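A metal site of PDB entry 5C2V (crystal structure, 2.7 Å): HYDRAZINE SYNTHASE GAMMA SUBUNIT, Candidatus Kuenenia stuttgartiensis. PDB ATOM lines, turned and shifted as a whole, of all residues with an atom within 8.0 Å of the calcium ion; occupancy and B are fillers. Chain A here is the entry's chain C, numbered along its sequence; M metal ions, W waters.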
ATOM      1  N   LYS A  92      -8.374   9.554  -3.779  1.00  0.00           N
ATOM      2  CA  LYS A  92      -7.742   8.252  -3.603  1.00  0.00           C
ATOM      3  C   LYS A  92      -7.345   7.969  -2.152  1.00  0.00           C
ATOM      4  O   LYS A  92      -6.841   8.834  -1.447  1.00  0.00           O
ATOM      5  CB  LYS A  92      -6.511   8.138  -4.496  1.00  0.00           C
ATOM      6  CG  LYS A  92      -6.737   7.319  -5.757  1.00  0.00           C
ATOM      7  CD  LYS A  92      -6.978   5.849  -5.422  1.00  0.00           C
ATOM      8  CE  LYS A  92      -7.152   5.007  -6.670  1.00  0.00           C
ATOM      9  NZ  LYS A  92      -7.387   3.570  -6.349  1.00  0.00           N
ATOM     10  N   GLY A  96      -1.062   2.026   1.834  1.00  0.00           N
ATOM     11  CA  GLY A  96      -0.575   0.904   1.052  1.00  0.00           C
ATOM     12  C   GLY A  96      -0.551   1.186  -0.441  1.00  0.00           C
ATOM     13  O   GLY A  96      -1.013   0.376  -1.244  1.00  0.00           O
ATOM     14  N   GLY A  97      -0.002   2.338  -0.810  1.00  0.00           N
ATOM     15  CA  GLY A  97      -0.019   2.785  -2.193  1.00  0.00           C
ATOM     16  C   GLY A  97       1.025   2.139  -3.085  1.00  0.00           C
ATOM     17  O   GLY A  97       0.788   1.945  -4.279  1.00  0.00           O
ATOM     18  N   TYR A  99       2.157  -0.876  -3.112  1.00  0.00           N
ATOM     19  CA  TYR A  99       1.953  -2.294  -3.379  1.00  0.00           C
ATOM     20  C   TYR A  99       1.170  -2.559  -4.665  1.00  0.00           C
ATOM     21  O   TYR A  99       1.192  -3.666  -5.191  1.00  0.00           O
ATOM     22  CB  TYR A  99       1.237  -2.951  -2.207  1.00  0.00           C
ATOM     23  CG  TYR A  99       2.039  -2.949  -0.925  1.00  0.00           C
ATOM     24  CD1 TYR A  99       3.427  -3.070  -0.959  1.00  0.00           C
ATOM     25  CD2 TYR A  99       1.432  -2.815   0.308  1.00  0.00           C
ATOM     26  CE1 TYR A  99       4.168  -3.069   0.211  1.00  0.00           C
ATOM     27  CE2 TYR A  99       2.161  -2.805   1.476  1.00  0.00           C
ATOM     28  CZ  TYR A  99       3.539  -2.931   1.421  1.00  0.00           C
ATOM     29  OH  TYR A  99       4.272  -2.929   2.585  1.00  0.00           O
ATOM     30  N   LEU A 100       0.488  -1.540  -5.178  1.00  0.00           N
ATOM     31  CA  LEU A 100      -0.348  -1.735  -6.362  1.00  0.00           C
ATOM     32  C   LEU A 100      -0.239  -0.624  -7.402  1.00  0.00           C
ATOM     33  O   LEU A 100      -1.118   0.243  -7.486  1.00  0.00           O
ATOM     34  CB  LEU A 100      -1.814  -1.886  -5.948  1.00  0.00           C
ATOM     35  CG  LEU A 100      -2.175  -3.213  -5.266  1.00  0.00           C
ATOM     36  CD1 LEU A 100      -3.582  -3.150  -4.720  1.00  0.00           C
ATOM     37  CD2 LEU A 100      -2.016  -4.370  -6.237  1.00  0.00           C
ATOM     38  N   PRO A 101       0.847  -0.641  -8.198  1.00  0.00           N
ATOM     39  CA  PRO A 101       0.969   0.166  -9.422  1.00  0.00           C
ATOM     40  C   PRO A 101       0.216  -0.500 -10.576  1.00  0.00           C
ATOM     41  O   PRO A 101      -0.002  -1.708 -10.525  1.00  0.00           O
ATOM     42  CB  PRO A 101       2.472   0.186  -9.668  1.00  0.00           C
ATOM     43  CG  PRO A 101       2.942  -1.109  -9.118  1.00  0.00           C
ATOM     44  CD  PRO A 101       2.081  -1.394  -7.921  1.00  0.00           C
ATOM     45  N   PRO A 102      -0.178   0.268 -11.611  1.00  0.00           N
ATOM     46  CA  PRO A 102       0.022   1.722 -11.737  1.00  0.00           C
ATOM     47  C   PRO A 102      -0.978   2.506 -10.897  1.00  0.00           C
ATOM     48  O   PRO A 102      -1.865   1.928 -10.273  1.00  0.00           O
ATOM     49  CB  PRO A 102      -0.208   1.970 -13.230  1.00  0.00           C
ATOM     50  CG  PRO A 102      -1.178   0.923 -13.618  1.00  0.00           C
ATOM     51  CD  PRO A 102      -0.835  -0.296 -12.801  1.00  0.00           C
ATOM     52  N   PHE A 103      -0.838   3.831 -10.907  1.00  0.00           N
ATOM     53  CA  PHE A 103      -1.549   4.673  -9.950  1.00  0.00           C
ATOM     54  C   PHE A 103      -2.727   5.442 -10.562  1.00  0.00           C
ATOM     55  O   PHE A 103      -3.077   5.249 -11.723  1.00  0.00           O
ATOM     56  CB  PHE A 103      -0.561   5.620  -9.287  1.00  0.00           C
ATOM     57  CG  PHE A 103       0.655   4.926  -8.748  1.00  0.00           C
ATOM     58  CD1 PHE A 103       0.560   4.083  -7.643  1.00  0.00           C
ATOM     59  CD2 PHE A 103       1.892   5.088  -9.347  1.00  0.00           C
ATOM     60  CE1 PHE A 103       1.669   3.431  -7.146  1.00  0.00           C
ATOM     61  CE2 PHE A 103       3.014   4.428  -8.849  1.00  0.00           C
ATOM     62  CZ  PHE A 103       2.899   3.606  -7.752  1.00  0.00           C
ATOM     63  N   ARG A 104      -3.302   6.323  -9.744  1.00  0.00           N
ATOM     64  CA  ARG A 104      -4.598   6.961 -10.002  1.00  0.00           C
ATOM     65  C   ARG A 104      -5.734   5.953 -10.171  1.00  0.00           C
ATOM     66  O   ARG A 104      -5.763   4.930  -9.495  1.00  0.00           O
ATOM     67  CB  ARG A 104      -4.522   7.863 -11.237  1.00  0.00           C
ATOM     68  CG  ARG A 104      -3.583   9.057 -11.110  1.00  0.00           C
ATOM     69  CD  ARG A 104      -4.358  10.347 -11.318  1.00  0.00           C
ATOM     70  NE  ARG A 104      -3.557  11.395 -11.948  1.00  0.00           N
ATOM     71  CZ  ARG A 104      -4.084  12.490 -12.497  1.00  0.00           C
ATOM     72  NH1 ARG A 104      -5.396  12.657 -12.497  1.00  0.00           N
ATOM     73  NH2 ARG A 104      -3.296  13.397 -13.047  1.00  0.00           N
ATOM     74  N   HIS A 105      -6.633   6.232 -11.103  1.00  0.00           N
ATOM     75  CA  HIS A 105      -7.836   5.430 -11.281  1.00  0.00           C
ATOM     76  C   HIS A 105      -7.890   4.830 -12.682  1.00  0.00           C
ATOM     77  O   HIS A 105      -7.889   3.610 -12.843  1.00  0.00           O
ATOM     78  CB  HIS A 105      -9.101   6.262 -11.022  1.00  0.00           C
ATOM     79  CG  HIS A 105      -9.499   6.319  -9.583  1.00  0.00           C
ATOM     80  ND1 HIS A 105      -9.188   7.388  -8.769  1.00  0.00           N
ATOM     81  CD2 HIS A 105     -10.186   5.455  -8.813  1.00  0.00           C
ATOM     82  CE1 HIS A 105      -9.668   7.176  -7.555  1.00  0.00           C
ATOM     83  NE2 HIS A 105     -10.277   6.004  -7.555  1.00  0.00           N
ATOM     84  N   GLU A 106      -7.974   5.694 -13.681  1.00  0.00           N
ATOM     85  CA  GLU A 106      -7.972   5.279 -15.079  1.00  0.00           C
ATOM     86  C   GLU A 106      -6.736   4.439 -15.388  1.00  0.00           C
ATOM     87  O   GLU A 106      -5.633   4.772 -14.969  1.00  0.00           O
ATOM     88  CB  GLU A 106      -8.039   6.492 -16.008  1.00  0.00           C
ATOM     89  CG  GLU A 106      -9.204   7.413 -15.711  1.00  0.00           C
ATOM     90  CD  GLU A 106      -9.314   8.557 -16.698  1.00  0.00           C
ATOM     91  OE1 GLU A 106      -8.422   8.691 -17.557  1.00  0.00           O
ATOM     92  OE2 GLU A 106     -10.297   9.323 -16.614  1.00  0.00           O
ATOM     93  N   ALA A 118      -3.034   5.234 -15.702  1.00  0.00           N
ATOM     94  CA  ALA A 118      -1.978   4.223 -15.626  1.00  0.00           C
ATOM     95  C   ALA A 118      -0.633   4.839 -15.236  1.00  0.00           C
ATOM     96  O   ALA A 118       0.385   4.557 -15.867  1.00  0.00           O
ATOM     97  CB  ALA A 118      -1.862   3.478 -16.945  1.00  0.00           C
ATOM     98  N   THR A 119      -0.651   5.678 -14.214  1.00  0.00           N
ATOM     99  CA  THR A 119       0.534   6.435 -13.822  1.00  0.00           C
ATOM    100  C   THR A 119       1.673   5.502 -13.403  1.00  0.00           C
ATOM    101  O   THR A 119       1.494   4.668 -12.512  1.00  0.00           O
ATOM    102  CB  THR A 119       0.219   7.414 -12.686  1.00  0.00           C
ATOM    103  OG1 THR A 119      -0.987   8.131 -12.988  1.00  0.00           O
ATOM    104  CG2 THR A 119       1.355   8.409 -12.515  1.00  0.00           C
ATOM    105  N   SER A 202      -6.319  -7.292  -5.218  1.00  0.00           N
ATOM    106  CA  SER A 202      -6.411  -6.632  -6.516  1.00  0.00           C
ATOM    107  C   SER A 202      -5.465  -7.281  -7.518  1.00  0.00           C
ATOM    108  O   SER A 202      -4.375  -7.721  -7.148  1.00  0.00           O
ATOM    109  CB  SER A 202      -6.096  -5.136  -6.389  1.00  0.00           C
ATOM    110  OG  SER A 202      -6.068  -4.498  -7.651  1.00  0.00           O
ATOM    111  N   ASP A 203      -5.868  -7.334  -8.782  1.00  0.00           N
ATOM    112  CA  ASP A 203      -5.030  -7.920  -9.823  1.00  0.00           C
ATOM    113  C   ASP A 203      -4.080  -6.891 -10.426  1.00  0.00           C
ATOM    114  O   ASP A 203      -3.228  -7.232 -11.244  1.00  0.00           O
ATOM    115  CB  ASP A 203      -5.888  -8.559 -10.921  1.00  0.00           C
ATOM    116  CG  ASP A 203      -6.901  -7.595 -11.518  1.00  0.00           C
ATOM    117  OD1 ASP A 203      -6.771  -6.369 -11.322  1.00  0.00           O
ATOM    118  OD2 ASP A 203      -7.837  -8.071 -12.205  1.00  0.00           O
ATOM    119  N   ALA A 204      -4.254  -5.640 -10.014  1.00  0.00           N
ATOM    120  CA  ALA A 204      -3.474  -4.512 -10.517  1.00  0.00           C
ATOM    121  C   ALA A 204      -3.576  -4.394 -12.034  1.00  0.00           C
ATOM    122  O   ALA A 204      -2.622  -4.013 -12.709  1.00  0.00           O
ATOM    123  CB  ALA A 204      -2.003  -4.646 -10.098  1.00  0.00           C
ATOM    124  N   GLN A 205      -4.752  -4.719 -12.567  1.00  0.00           N
ATOM    125  CA  GLN A 205      -4.995  -4.638 -13.999  1.00  0.00           C
ATOM    126  C   GLN A 205      -6.107  -3.644 -14.333  1.00  0.00           C
ATOM    127  O   GLN A 205      -6.695  -3.043 -13.441  1.00  0.00           O
ATOM    128  CB  GLN A 205      -5.338  -6.012 -14.565  1.00  0.00           C
ATOM    129  CG  GLN A 205      -4.257  -7.064 -14.370  1.00  0.00           C
ATOM    130  CD  GLN A 205      -4.633  -8.413 -14.963  1.00  0.00           C
ATOM    131  OE1 GLN A 205      -5.523  -8.493 -15.811  1.00  0.00           O
ATOM    132  NE2 GLN A 205      -3.966  -9.462 -14.519  1.00  0.00           N
ATOM    133  N   ASP A 257      -8.241   1.019 -13.398  1.00  0.00           N
ATOM    134  CA  ASP A 257      -7.331   0.225 -12.586  1.00  0.00           C
ATOM    135  C   ASP A 257      -8.011  -0.201 -11.285  1.00  0.00           C
ATOM    136  O   ASP A 257      -8.542   0.636 -10.556  1.00  0.00           O
ATOM    137  CB  ASP A 257      -6.049   1.003 -12.303  1.00  0.00           C
ATOM    138  CG  ASP A 257      -5.207   0.388 -11.198  1.00  0.00           C
ATOM    139  OD1 ASP A 257      -4.616  -0.683 -11.430  1.00  0.00           O
ATOM    140  OD2 ASP A 257      -5.132   0.990 -10.108  1.00  0.00           O
ATOM    141  N   THR A 258      -8.003  -1.495 -10.997  1.00  0.00           N
ATOM    142  CA  THR A 258      -8.681  -2.030  -9.826  1.00  0.00           C
ATOM    143  C   THR A 258      -7.971  -1.670  -8.525  1.00  0.00           C
ATOM    144  O   THR A 258      -6.775  -1.934  -8.375  1.00  0.00           O
ATOM    145  CB  THR A 258      -8.827  -3.562  -9.901  1.00  0.00           C
ATOM    146  OG1 THR A 258      -7.611  -4.188  -9.448  1.00  0.00           O
ATOM    147  CG2 THR A 258      -9.140  -4.003 -11.314  1.00  0.00           C
ATOM    148  N   PRO A 259      -8.703  -1.063  -7.586  1.00  0.00           N
ATOM    149  CA  PRO A 259      -8.197  -0.698  -6.256  1.00  0.00           C
ATOM    150  C   PRO A 259      -8.131  -1.898  -5.307  1.00  0.00           C
ATOM    151  O   PRO A 259      -8.818  -2.890  -5.529  1.00  0.00           O
ATOM    152  CB  PRO A 259      -9.220   0.324  -5.756  1.00  0.00           C
ATOM    153  CG  PRO A 259     -10.135   0.611  -6.920  1.00  0.00           C
ATOM    154  CD  PRO A 259     -10.082  -0.595  -7.783  1.00  0.00           C
ATOM    155  N   THR A 260      -7.319  -1.778  -4.270  1.00  0.00           N
ATOM    156  CA  THR A 260      -7.281  -2.794  -3.216  1.00  0.00           C
ATOM    157  C   THR A 260      -8.601  -2.812  -2.452  1.00  0.00           C
ATOM    158  O   THR A 260      -9.307  -1.800  -2.392  1.00  0.00           O
ATOM    159  CB  THR A 260      -6.129  -2.539  -2.220  1.00  0.00           C
ATOM    160  OG1 THR A 260      -6.146  -3.553  -1.209  1.00  0.00           O
ATOM    161  CG2 THR A 260      -6.277  -1.178  -1.567  1.00  0.00           C
HETATM  162 CA    CA M   1      -3.171   0.677  -8.785  1.00  0.00          CA
HETATM  163  O   HOH W   1      -4.495  -0.557  -7.228  1.00  0.00           O
HETATM  164  O   HOH W   2      -3.634   2.675  -7.550  1.00  0.00           O
HETATM  165  O   HOH W   3      -2.732  -1.320 -10.019  1.00  0.00           O
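Three residues have an atom within 4 Å of the calcium ion: Leu 100, Pro 102 and Asp 257. Along chain A the residues within 4 Å of the calcium ion span positions 100 to 257.
The calcium ion is bound by the backbone carbonyl oxygen (O) of Pro 102 (2.3 Å). The calcium ion is bound by OD2 of Asp 257, 2.4 Å away. Water W3 binds the calcium ion, at 2.4 Å. The calcium ion is bound by water W1, at 2.4 Å. Water W2 is bound to the calcium ion, 2.4 Å away. O of Leu 100 binds the calcium ion, 2.5 Å away.
Water W3 bridges OD1 of Asp 257 and O of Pro 101.
N of Asp 257 is in hydrogen-bond range of O of His 105, 2.7 Å away.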
